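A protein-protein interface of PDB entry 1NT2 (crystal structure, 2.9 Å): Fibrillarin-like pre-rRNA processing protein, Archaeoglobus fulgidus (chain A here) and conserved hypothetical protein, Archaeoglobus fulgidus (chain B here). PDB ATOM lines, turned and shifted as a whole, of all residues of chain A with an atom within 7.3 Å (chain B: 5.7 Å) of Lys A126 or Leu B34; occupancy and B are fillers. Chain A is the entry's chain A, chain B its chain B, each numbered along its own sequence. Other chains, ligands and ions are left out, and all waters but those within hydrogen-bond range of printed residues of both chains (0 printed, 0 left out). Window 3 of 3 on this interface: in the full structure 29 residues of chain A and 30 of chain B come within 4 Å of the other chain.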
ATOM      1  N   ARG A  60      23.016  -3.054  -8.921  1.00  0.00           N
ATOM      2  CA  ARG A  60      23.048  -2.289 -10.172  1.00  0.00           C
ATOM      3  C   ARG A  60      21.625  -1.918 -10.539  1.00  0.00           C
ATOM      4  O   ARG A  60      20.881  -2.748 -11.076  1.00  0.00           O
ATOM      5  CB  ARG A  60      23.657  -3.115 -11.316  1.00  0.00           C
ATOM      6  CG  ARG A  60      25.122  -2.810 -11.601  1.00  0.00           C
ATOM      7  CD  ARG A  60      25.986  -3.157 -10.405  1.00  0.00           C
ATOM      8  NE  ARG A  60      27.241  -2.411 -10.383  1.00  0.00           N
ATOM      9  CZ  ARG A  60      27.988  -2.262  -9.292  1.00  0.00           C
ATOM     10  NH1 ARG A  60      27.592  -2.814  -8.150  1.00  0.00           N
ATOM     11  NH2 ARG A  60      29.118  -1.556  -9.335  1.00  0.00           N
ATOM     12  N   VAL A  61      21.260  -0.665 -10.277  1.00  0.00           N
ATOM     13  CA  VAL A  61      19.906  -0.190 -10.545  1.00  0.00           C
ATOM     14  C   VAL A  61      19.650   0.673 -11.784  1.00  0.00           C
ATOM     15  O   VAL A  61      20.399   1.606 -12.104  1.00  0.00           O
ATOM     16  CB  VAL A  61      19.368   0.583  -9.336  1.00  0.00           C
ATOM     17  CG1 VAL A  61      17.869   0.753  -9.460  1.00  0.00           C
ATOM     18  CG2 VAL A  61      19.727  -0.144  -8.067  1.00  0.00           C
ATOM     19  N   TYR A  85      21.399   4.049 -12.702  1.00  0.00           N
ATOM     20  CA  TYR A  85      21.317   4.668 -14.032  1.00  0.00           C
ATOM     21  C   TYR A  85      19.935   5.305 -14.150  1.00  0.00           C
ATOM     22  O   TYR A  85      19.003   4.683 -14.654  1.00  0.00           O
ATOM     23  CB  TYR A  85      21.485   3.628 -15.155  1.00  0.00           C
ATOM     24  CG  TYR A  85      22.819   2.896 -15.199  1.00  0.00           C
ATOM     25  CD1 TYR A  85      22.976   1.654 -14.590  1.00  0.00           C
ATOM     26  CD2 TYR A  85      23.915   3.435 -15.872  1.00  0.00           C
ATOM     27  CE1 TYR A  85      24.187   0.966 -14.654  1.00  0.00           C
ATOM     28  CE2 TYR A  85      25.127   2.754 -15.939  1.00  0.00           C
ATOM     29  CZ  TYR A  85      25.254   1.521 -15.328  1.00  0.00           C
ATOM     30  OH  TYR A  85      26.446   0.831 -15.398  1.00  0.00           O
ATOM     31  N   SER A 121      21.416   1.575 -24.963  1.00  0.00           N
ATOM     32  CA  SER A 121      21.812   0.196 -24.693  1.00  0.00           C
ATOM     33  C   SER A 121      23.309   0.000 -24.534  1.00  0.00           C
ATOM     34  O   SER A 121      23.748  -1.015 -23.999  1.00  0.00           O
ATOM     35  CB  SER A 121      21.335  -0.724 -25.815  1.00  0.00           C
ATOM     36  OG  SER A 121      22.355  -0.891 -26.784  1.00  0.00           O
ATOM     37  N   GLY A 122      24.099   0.946 -25.025  1.00  0.00           N
ATOM     38  CA  GLY A 122      25.539   0.812 -24.894  1.00  0.00           C
ATOM     39  C   GLY A 122      26.105   1.553 -23.689  1.00  0.00           C
ATOM     40  O   GLY A 122      27.308   1.830 -23.634  1.00  0.00           O
ATOM     41  N   ILE A 123      25.239   1.875 -22.728  1.00  0.00           N
ATOM     42  CA  ILE A 123      25.640   2.600 -21.525  1.00  0.00           C
ATOM     43  C   ILE A 123      25.198   1.817 -20.301  1.00  0.00           C
ATOM     44  O   ILE A 123      25.929   1.688 -19.317  1.00  0.00           O
ATOM     45  CB  ILE A 123      24.975   4.004 -21.451  1.00  0.00           C
ATOM     46  CG1 ILE A 123      25.402   4.865 -22.641  1.00  0.00           C
ATOM     47  CG2 ILE A 123      25.361   4.695 -20.149  1.00  0.00           C
ATOM     48  CD1 ILE A 123      24.786   6.246 -22.645  1.00  0.00           C
ATOM     49  N   VAL A 124      23.983   1.301 -20.366  1.00  0.00           N
ATOM     50  CA  VAL A 124      23.447   0.545 -19.256  1.00  0.00           C
ATOM     51  C   VAL A 124      23.999  -0.872 -19.274  1.00  0.00           C
ATOM     52  O   VAL A 124      24.017  -1.528 -20.314  1.00  0.00           O
ATOM     53  CB  VAL A 124      21.913   0.509 -19.319  1.00  0.00           C
ATOM     54  CG1 VAL A 124      21.358  -0.255 -18.139  1.00  0.00           C
ATOM     55  CG2 VAL A 124      21.378   1.929 -19.336  1.00  0.00           C
ATOM     56  N   GLU A 125      24.470  -1.329 -18.119  1.00  0.00           N
ATOM     57  CA  GLU A 125      25.008  -2.674 -17.993  1.00  0.00           C
ATOM     58  C   GLU A 125      23.875  -3.599 -17.589  1.00  0.00           C
ATOM     59  O   GLU A 125      22.721  -3.176 -17.512  1.00  0.00           O
ATOM     60  CB  GLU A 125      26.089  -2.720 -16.922  1.00  0.00           C
ATOM     61  CG  GLU A 125      25.580  -2.567 -15.508  1.00  0.00           C
ATOM     62  CD  GLU A 125      26.692  -2.733 -14.494  1.00  0.00           C
ATOM     63  OE1 GLU A 125      27.546  -1.822 -14.390  1.00  0.00           O
ATOM     64  OE2 GLU A 125      26.713  -3.786 -13.816  1.00  0.00           O
ATOM     65  N   LYS A 126      24.192  -4.864 -17.337  1.00  0.00           N
ATOM     66  CA  LYS A 126      23.159  -5.796 -16.915  1.00  0.00           C
ATOM     67  C   LYS A 126      22.802  -5.368 -15.498  1.00  0.00           C
ATOM     68  O   LYS A 126      23.655  -5.353 -14.612  1.00  0.00           O
ATOM     69  CB  LYS A 126      23.685  -7.231 -16.948  1.00  0.00           C
ATOM     70  CG  LYS A 126      23.960  -7.756 -18.353  1.00  0.00           C
ATOM     71  CD  LYS A 126      22.686  -7.844 -19.169  1.00  0.00           C
ATOM     72  CE  LYS A 126      22.944  -8.457 -20.536  1.00  0.00           C
ATOM     73  NZ  LYS A 126      21.691  -8.580 -21.352  1.00  0.00           N
ATOM     74  N   VAL A 127      21.544  -4.988 -15.307  1.00  0.00           N
ATOM     75  CA  VAL A 127      21.061  -4.523 -14.015  1.00  0.00           C
ATOM     76  C   VAL A 127      20.350  -5.618 -13.212  1.00  0.00           C
ATOM     77  O   VAL A 127      19.778  -6.563 -13.785  1.00  0.00           O
ATOM     78  CB  VAL A 127      20.104  -3.317 -14.201  1.00  0.00           C
ATOM     79  CG1 VAL A 127      20.845  -2.169 -14.852  1.00  0.00           C
ATOM     80  CG2 VAL A 127      18.910  -3.715 -15.067  1.00  0.00           C
ATOM     81  N   ASP A 128      20.391  -5.467 -11.884  1.00  0.00           N
ATOM     82  CA  ASP A 128      19.786  -6.412 -10.939  1.00  0.00           C
ATOM     83  C   ASP A 128      18.308  -6.122 -10.681  1.00  0.00           C
ATOM     84  O   ASP A 128      17.573  -6.964 -10.144  1.00  0.00           O
ATOM     85  CB  ASP A 128      20.527  -6.354  -9.607  1.00  0.00           C
ATOM     86  CG  ASP A 128      22.014  -6.566  -9.761  1.00  0.00           C
ATOM     87  OD1 ASP A 128      22.397  -7.574 -10.392  1.00  0.00           O
ATOM     88  OD2 ASP A 128      22.794  -5.732  -9.241  1.00  0.00           O
ATOM     89  N   LEU A 129      17.890  -4.913 -11.048  1.00  0.00           N
ATOM     90  CA  LEU A 129      16.510  -4.475 -10.864  1.00  0.00           C
ATOM     91  C   LEU A 129      16.183  -3.205 -11.646  1.00  0.00           C
ATOM     92  O   LEU A 129      16.981  -2.256 -11.689  1.00  0.00           O
ATOM     93  CB  LEU A 129      16.219  -4.264  -9.374  1.00  0.00           C
ATOM     94  CG  LEU A 129      15.266  -3.137  -8.985  1.00  0.00           C
ATOM     95  CD1 LEU A 129      14.307  -3.608  -7.912  1.00  0.00           C
ATOM     96  CD2 LEU A 129      16.080  -1.942  -8.521  1.00  0.00           C
ATOM     97  N   ALA A 147      13.506  -4.434 -19.893  1.00  0.00           N
ATOM     98  CA  ALA A 147      13.913  -5.655 -19.197  1.00  0.00           C
ATOM     99  C   ALA A 147      14.755  -6.547 -20.117  1.00  0.00           C
ATOM    100  O   ALA A 147      15.810  -7.050 -19.722  1.00  0.00           O
ATOM    101  CB  ALA A 147      12.669  -6.419 -18.712  1.00  0.00           C
ATOM    102  N   GLU A 148      14.274  -6.736 -21.341  1.00  0.00           N
ATOM    103  CA  GLU A 148      14.972  -7.553 -22.319  1.00  0.00           C
ATOM    104  C   GLU A 148      16.424  -7.110 -22.357  1.00  0.00           C
ATOM    105  O   GLU A 148      17.340  -7.872 -22.038  1.00  0.00           O
ATOM    106  CB  GLU A 148      14.363  -7.355 -23.703  1.00  0.00           C
ATOM    107  CG  GLU A 148      14.634  -8.498 -24.674  1.00  0.00           C
ATOM    108  CD  GLU A 148      13.512  -9.540 -24.683  1.00  0.00           C
ATOM    109  OE1 GLU A 148      13.662 -10.582 -25.368  1.00  0.00           O
ATOM    110  OE2 GLU A 148      12.477  -9.306 -24.010  1.00  0.00           O
ATOM    111  N   PHE A 149      16.617  -5.856 -22.736  1.00  0.00           N
ATOM    112  CA  PHE A 149      17.948  -5.279 -22.837  1.00  0.00           C
ATOM    113  C   PHE A 149      18.875  -5.410 -21.640  1.00  0.00           C
ATOM    114  O   PHE A 149      20.015  -5.833 -21.802  1.00  0.00           O
ATOM    115  CB  PHE A 149      17.862  -3.796 -23.212  1.00  0.00           C
ATOM    116  CG  PHE A 149      17.785  -3.554 -24.686  1.00  0.00           C
ATOM    117  CD1 PHE A 149      16.651  -3.926 -25.410  1.00  0.00           C
ATOM    118  CD2 PHE A 149      18.850  -2.970 -25.362  1.00  0.00           C
ATOM    119  CE1 PHE A 149      16.575  -3.720 -26.791  1.00  0.00           C
ATOM    120  CE2 PHE A 149      18.789  -2.761 -26.741  1.00  0.00           C
ATOM    121  CZ  PHE A 149      17.647  -3.137 -27.457  1.00  0.00           C
ATOM    122  N   PHE A 150      18.403  -5.076 -20.442  1.00  0.00           N
ATOM    123  CA  PHE A 150      19.303  -5.097 -19.294  1.00  0.00           C
ATOM    124  C   PHE A 150      18.989  -5.957 -18.061  1.00  0.00           C
ATOM    125  O   PHE A 150      19.897  -6.319 -17.308  1.00  0.00           O
ATOM    126  CB  PHE A 150      19.534  -3.642 -18.868  1.00  0.00           C
ATOM    127  CG  PHE A 150      19.620  -2.681 -20.029  1.00  0.00           C
ATOM    128  CD1 PHE A 150      20.658  -2.761 -20.940  1.00  0.00           C
ATOM    129  CD2 PHE A 150      18.635  -1.732 -20.237  1.00  0.00           C
ATOM    130  CE1 PHE A 150      20.707  -1.913 -22.039  1.00  0.00           C
ATOM    131  CE2 PHE A 150      18.677  -0.876 -21.336  1.00  0.00           C
ATOM    132  CZ  PHE A 150      19.710  -0.969 -22.236  1.00  0.00           C
ATOM    133  N   LEU A 151      17.725  -6.287 -17.840  1.00  0.00           N
ATOM    134  CA  LEU A 151      17.394  -7.082 -16.666  1.00  0.00           C
ATOM    135  C   LEU A 151      18.006  -8.477 -16.721  1.00  0.00           C
ATOM    136  O   LEU A 151      17.479  -9.384 -17.378  1.00  0.00           O
ATOM    137  CB  LEU A 151      15.880  -7.200 -16.486  1.00  0.00           C
ATOM    138  CG  LEU A 151      15.484  -8.139 -15.340  1.00  0.00           C
ATOM    139  CD1 LEU A 151      16.008  -7.595 -14.023  1.00  0.00           C
ATOM    140  CD2 LEU A 151      13.987  -8.286 -15.301  1.00  0.00           C
ATOM    141  N   LYS A 152      19.115  -8.644 -16.006  1.00  0.00           N
ATOM    142  CA  LYS A 152      19.815  -9.920 -15.953  1.00  0.00           C
ATOM    143  C   LYS A 152      18.914 -11.060 -15.448  1.00  0.00           C
ATOM    144  O   LYS A 152      18.204 -10.908 -14.455  1.00  0.00           O
ATOM    145  CB  LYS A 152      21.045  -9.776 -15.058  1.00  0.00           C
ATOM    146  CG  LYS A 152      20.710  -9.456 -13.627  1.00  0.00           C
ATOM    147  CD  LYS A 152      21.798  -8.651 -12.963  1.00  0.00           C
ATOM    148  CE  LYS A 152      23.148  -9.313 -13.069  1.00  0.00           C
ATOM    149  NZ  LYS A 152      24.181  -8.572 -12.290  1.00  0.00           N
ATOM    150  N   GLU A 153      18.952 -12.197 -16.145  1.00  0.00           N
ATOM    151  CA  GLU A 153      18.153 -13.378 -15.791  1.00  0.00           C
ATOM    152  C   GLU A 153      18.056 -13.568 -14.290  1.00  0.00           C
ATOM    153  O   GLU A 153      19.067 -13.633 -13.590  1.00  0.00           O
ATOM    154  CB  GLU A 153      18.742 -14.655 -16.418  1.00  0.00           C
ATOM    155  CG  GLU A 153      18.017 -15.138 -17.683  1.00  0.00           C
ATOM    156  CD  GLU A 153      17.750 -16.649 -17.693  1.00  0.00           C
ATOM    157  OE1 GLU A 153      17.128 -17.137 -18.662  1.00  0.00           O
ATOM    158  OE2 GLU A 153      18.154 -17.349 -16.736  1.00  0.00           O
ATOM    159  N   TYR B   3      30.081  -3.089 -32.042  1.00  0.00           N
ATOM    160  CA  TYR B   3      29.266  -2.730 -30.892  1.00  0.00           C
ATOM    161  C   TYR B   3      29.633  -1.309 -30.484  1.00  0.00           C
ATOM    162  O   TYR B   3      30.803  -0.941 -30.486  1.00  0.00           O
ATOM    163  CB  TYR B   3      29.501  -3.708 -29.739  1.00  0.00           C
ATOM    164  CG  TYR B   3      28.812  -5.048 -29.914  1.00  0.00           C
ATOM    165  CD1 TYR B   3      29.549  -6.233 -30.011  1.00  0.00           C
ATOM    166  CD2 TYR B   3      27.423  -5.135 -29.937  1.00  0.00           C
ATOM    167  CE1 TYR B   3      28.916  -7.469 -30.118  1.00  0.00           C
ATOM    168  CE2 TYR B   3      26.781  -6.363 -30.043  1.00  0.00           C
ATOM    169  CZ  TYR B   3      27.527  -7.527 -30.130  1.00  0.00           C
ATOM    170  OH  TYR B   3      26.875  -8.740 -30.203  1.00  0.00           O
ATOM    171  N   LEU B   5      29.733   1.002 -27.510  1.00  0.00           N
ATOM    172  CA  LEU B   5      29.644   1.221 -26.076  1.00  0.00           C
ATOM    173  C   LEU B   5      30.069   2.659 -25.803  1.00  0.00           C
ATOM    174  O   LEU B   5      30.711   3.283 -26.643  1.00  0.00           O
ATOM    175  CB  LEU B   5      30.547   0.236 -25.347  1.00  0.00           C
ATOM    176  CG  LEU B   5      30.467  -1.203 -25.872  1.00  0.00           C
ATOM    177  CD1 LEU B   5      31.181  -2.119 -24.883  1.00  0.00           C
ATOM    178  CD2 LEU B   5      29.015  -1.642 -26.070  1.00  0.00           C
ATOM    179  N   ASN B  30      22.920   0.626 -30.390  1.00  0.00           N
ATOM    180  CA  ASN B  30      22.925  -0.821 -30.531  1.00  0.00           C
ATOM    181  C   ASN B  30      21.461  -1.186 -30.614  1.00  0.00           C
ATOM    182  O   ASN B  30      20.701  -0.845 -29.720  1.00  0.00           O
ATOM    183  CB  ASN B  30      23.575  -1.471 -29.314  1.00  0.00           C
ATOM    184  CG  ASN B  30      25.089  -1.396 -29.352  1.00  0.00           C
ATOM    185  OD1 ASN B  30      25.725  -2.025 -30.189  1.00  0.00           O
ATOM    186  ND2 ASN B  30      25.671  -0.625 -28.447  1.00  0.00           N
ATOM    187  N   SER B  32      20.027  -4.181 -30.448  1.00  0.00           N
ATOM    188  CA  SER B  32      19.684  -5.481 -29.909  1.00  0.00           C
ATOM    189  C   SER B  32      20.491  -5.768 -28.657  1.00  0.00           C
ATOM    190  O   SER B  32      21.706  -5.556 -28.636  1.00  0.00           O
ATOM    191  CB  SER B  32      19.962  -6.547 -30.974  1.00  0.00           C
ATOM    192  OG  SER B  32      19.733  -7.858 -30.486  1.00  0.00           O
ATOM    193  N   PRO B  33      19.830  -6.271 -27.600  1.00  0.00           N
ATOM    194  CA  PRO B  33      20.490  -6.592 -26.334  1.00  0.00           C
ATOM    195  C   PRO B  33      21.945  -7.002 -26.551  1.00  0.00           C
ATOM    196  O   PRO B  33      22.249  -7.706 -27.516  1.00  0.00           O
ATOM    197  CB  PRO B  33      19.639  -7.737 -25.800  1.00  0.00           C
ATOM    198  CG  PRO B  33      18.272  -7.341 -26.222  1.00  0.00           C
ATOM    199  CD  PRO B  33      18.477  -6.857 -27.644  1.00  0.00           C
ATOM    200  N   LEU B  34      22.848  -6.561 -25.682  1.00  0.00           N
ATOM    201  CA  LEU B  34      24.249  -6.935 -25.841  1.00  0.00           C
ATOM    202  C   LEU B  34      24.498  -8.310 -25.218  1.00  0.00           C
ATOM    203  O   LEU B  34      23.822  -8.687 -24.254  1.00  0.00           O
ATOM    204  CB  LEU B  34      25.160  -5.892 -25.200  1.00  0.00           C
ATOM    205  CG  LEU B  34      25.029  -4.454 -25.706  1.00  0.00           C
ATOM    206  CD1 LEU B  34      26.303  -3.693 -25.360  1.00  0.00           C
ATOM    207  CD2 LEU B  34      24.810  -4.437 -27.205  1.00  0.00           C
ATOM    208  N   PRO B  35      25.450  -9.092 -25.775  1.00  0.00           N
ATOM    209  CA  PRO B  35      25.710 -10.418 -25.200  1.00  0.00           C
ATOM    210  C   PRO B  35      26.812 -10.362 -24.156  1.00  0.00           C
ATOM    211  O   PRO B  35      27.365 -11.389 -23.776  1.00  0.00           O
ATOM    212  CB  PRO B  35      26.117 -11.263 -26.412  1.00  0.00           C
ATOM    213  CG  PRO B  35      25.734 -10.411 -27.621  1.00  0.00           C
ATOM    214  CD  PRO B  35      26.002  -9.019 -27.135  1.00  0.00           C
ATOM    215  N   PHE B  36      27.124  -9.153 -23.702  1.00  0.00           N
ATOM    216  CA  PHE B  36      28.154  -8.952 -22.691  1.00  0.00           C
ATOM    217  C   PHE B  36      27.866  -7.789 -21.749  1.00  0.00           C
ATOM    218  O   PHE B  36      26.955  -6.993 -21.987  1.00  0.00           O
ATOM    219  CB  PHE B  36      29.504  -8.733 -23.354  1.00  0.00           C
ATOM    220  CG  PHE B  36      29.473  -7.759 -24.485  1.00  0.00           C
ATOM    221  CD1 PHE B  36      28.791  -8.060 -25.655  1.00  0.00           C
ATOM    222  CD2 PHE B  36      30.177  -6.557 -24.398  1.00  0.00           C
ATOM    223  CE1 PHE B  36      28.818  -7.178 -26.731  1.00  0.00           C
ATOM    224  CE2 PHE B  36      30.214  -5.662 -25.465  1.00  0.00           C
ATOM    225  CZ  PHE B  36      29.539  -5.967 -26.636  1.00  0.00           C
ATOM    226  N   ASN B  37      28.640  -7.691 -20.674  1.00  0.00           N
ATOM    227  CA  ASN B  37      28.439  -6.612 -19.715  1.00  0.00           C
ATOM    228  C   ASN B  37      29.306  -5.430 -20.039  1.00  0.00           C
ATOM    229  O   ASN B  37      30.503  -5.444 -19.756  1.00  0.00           O
ATOM    230  CB  ASN B  37      28.752  -7.070 -18.296  1.00  0.00           C
ATOM    231  CG  ASN B  37      27.523  -7.556 -17.560  1.00  0.00           C
ATOM    232  OD1 ASN B  37      26.861  -8.512 -17.987  1.00  0.00           O
ATOM    233  ND2 ASN B  37      27.204  -6.897 -16.446  1.00  0.00           N
ATOM    234  N   VAL B  38      28.702  -4.405 -20.629  1.00  0.00           N
ATOM    235  CA  VAL B  38      29.445  -3.205 -20.991  1.00  0.00           C
ATOM    236  C   VAL B  38      30.326  -2.784 -19.821  1.00  0.00           C
ATOM    237  O   VAL B  38      31.450  -2.309 -19.999  1.00  0.00           O
ATOM    238  CB  VAL B  38      28.494  -2.050 -21.332  1.00  0.00           C
ATOM    239  CG1 VAL B  38      29.291  -0.863 -21.882  1.00  0.00           C
ATOM    240  CG2 VAL B  38      27.449  -2.528 -22.324  1.00  0.00           C
ATOM    241  N   SER B  39      29.792  -2.973 -18.623  1.00  0.00           N
ATOM    242  CA  SER B  39      30.490  -2.643 -17.399  1.00  0.00           C
ATOM    243  C   SER B  39      31.814  -3.400 -17.308  1.00  0.00           C
ATOM    244  O   SER B  39      32.857  -2.804 -17.037  1.00  0.00           O
ATOM    245  CB  SER B  39      29.604  -2.996 -16.204  1.00  0.00           C
ATOM    246  OG  SER B  39      29.058  -4.300 -16.354  1.00  0.00           O
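The guanidinium group (NE) of Arg A60 is in salt-bridge range of the side-chain carboxylate (OE2) of Glu A125 (3.7 Å). OH of Tyr A85 sits at hydrogen-bond distance from OE1 of Glu A125, 3.0 Å away. NZ of Lys A126 sits at hydrogen-bond distance from O of Phe A149 (3.2 Å). The side-chain amide nitrogen (ND2) of Asn B37 is in hydrogen-bond range of the side-chain hydroxyl (OG) of Ser B39 (3.2 Å).
Lys A126 touches just these residues of chain B: Leu B34 (3.6 Å) and Asn B37 (3.0 Å). Of chain A, only Ser A121 and Lys A126 come within 4 Å of Leu B34. Of the printed residues of chain A, Ser B39 touches Glu A125 (3.0 Å). Printed residues of chain A within 4 Å of Ser B32: Phe A149. Tyr A85 touches none of the printed residues of chain B. Asp A128 touches none of the printed residues of chain B. The nearest residue of chain B that does not touch Lys A126 is Phe B36 (4.5 Å). The nearest printed residue of chain A that does not touch Ser B32 is Ser A121 (5.1 Å).
OG of Ser A121 lies close to O of Asn B30, at 3.4 Å. The side-chain carboxylate (OE2) of Glu A125 lies close to the side-chain hydroxyl (OG) of Ser B39 (3.5 Å).
Hydrophobic or aromatic side chains of chain B that line the printed part of chain A: Leu B5, Pro B33, Leu B34 and Val B38. Hydrophobic or aromatic side chains of chain A that line the printed part of chain B: Phe A149. Among the printed residues, 10 pairs touch across the chains. Among the printed residues, no Asp or Glu carboxylate lies within 4 Å of a Lys or Arg side-chain nitrogen of the other chain.
Ser A121 touches Leu B34. Gly A122 touches Leu B5. ND2 of Asn B30 touches CA of Gly A122, 3.8 Å away. Gly A122 touches Val B38 (O to CG1, 3.8 Å). NZ of Lys A126 touches O of Leu B34, 3.6 Å away. OD1 of Asn B37 touches CG of Lys A126, 3.0 Å away. Phe A149 touches Ser B32 (CE2 to C, 3.95 Å). CE2 of Phe A149 touches N of Pro B33 (3.8 Å).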
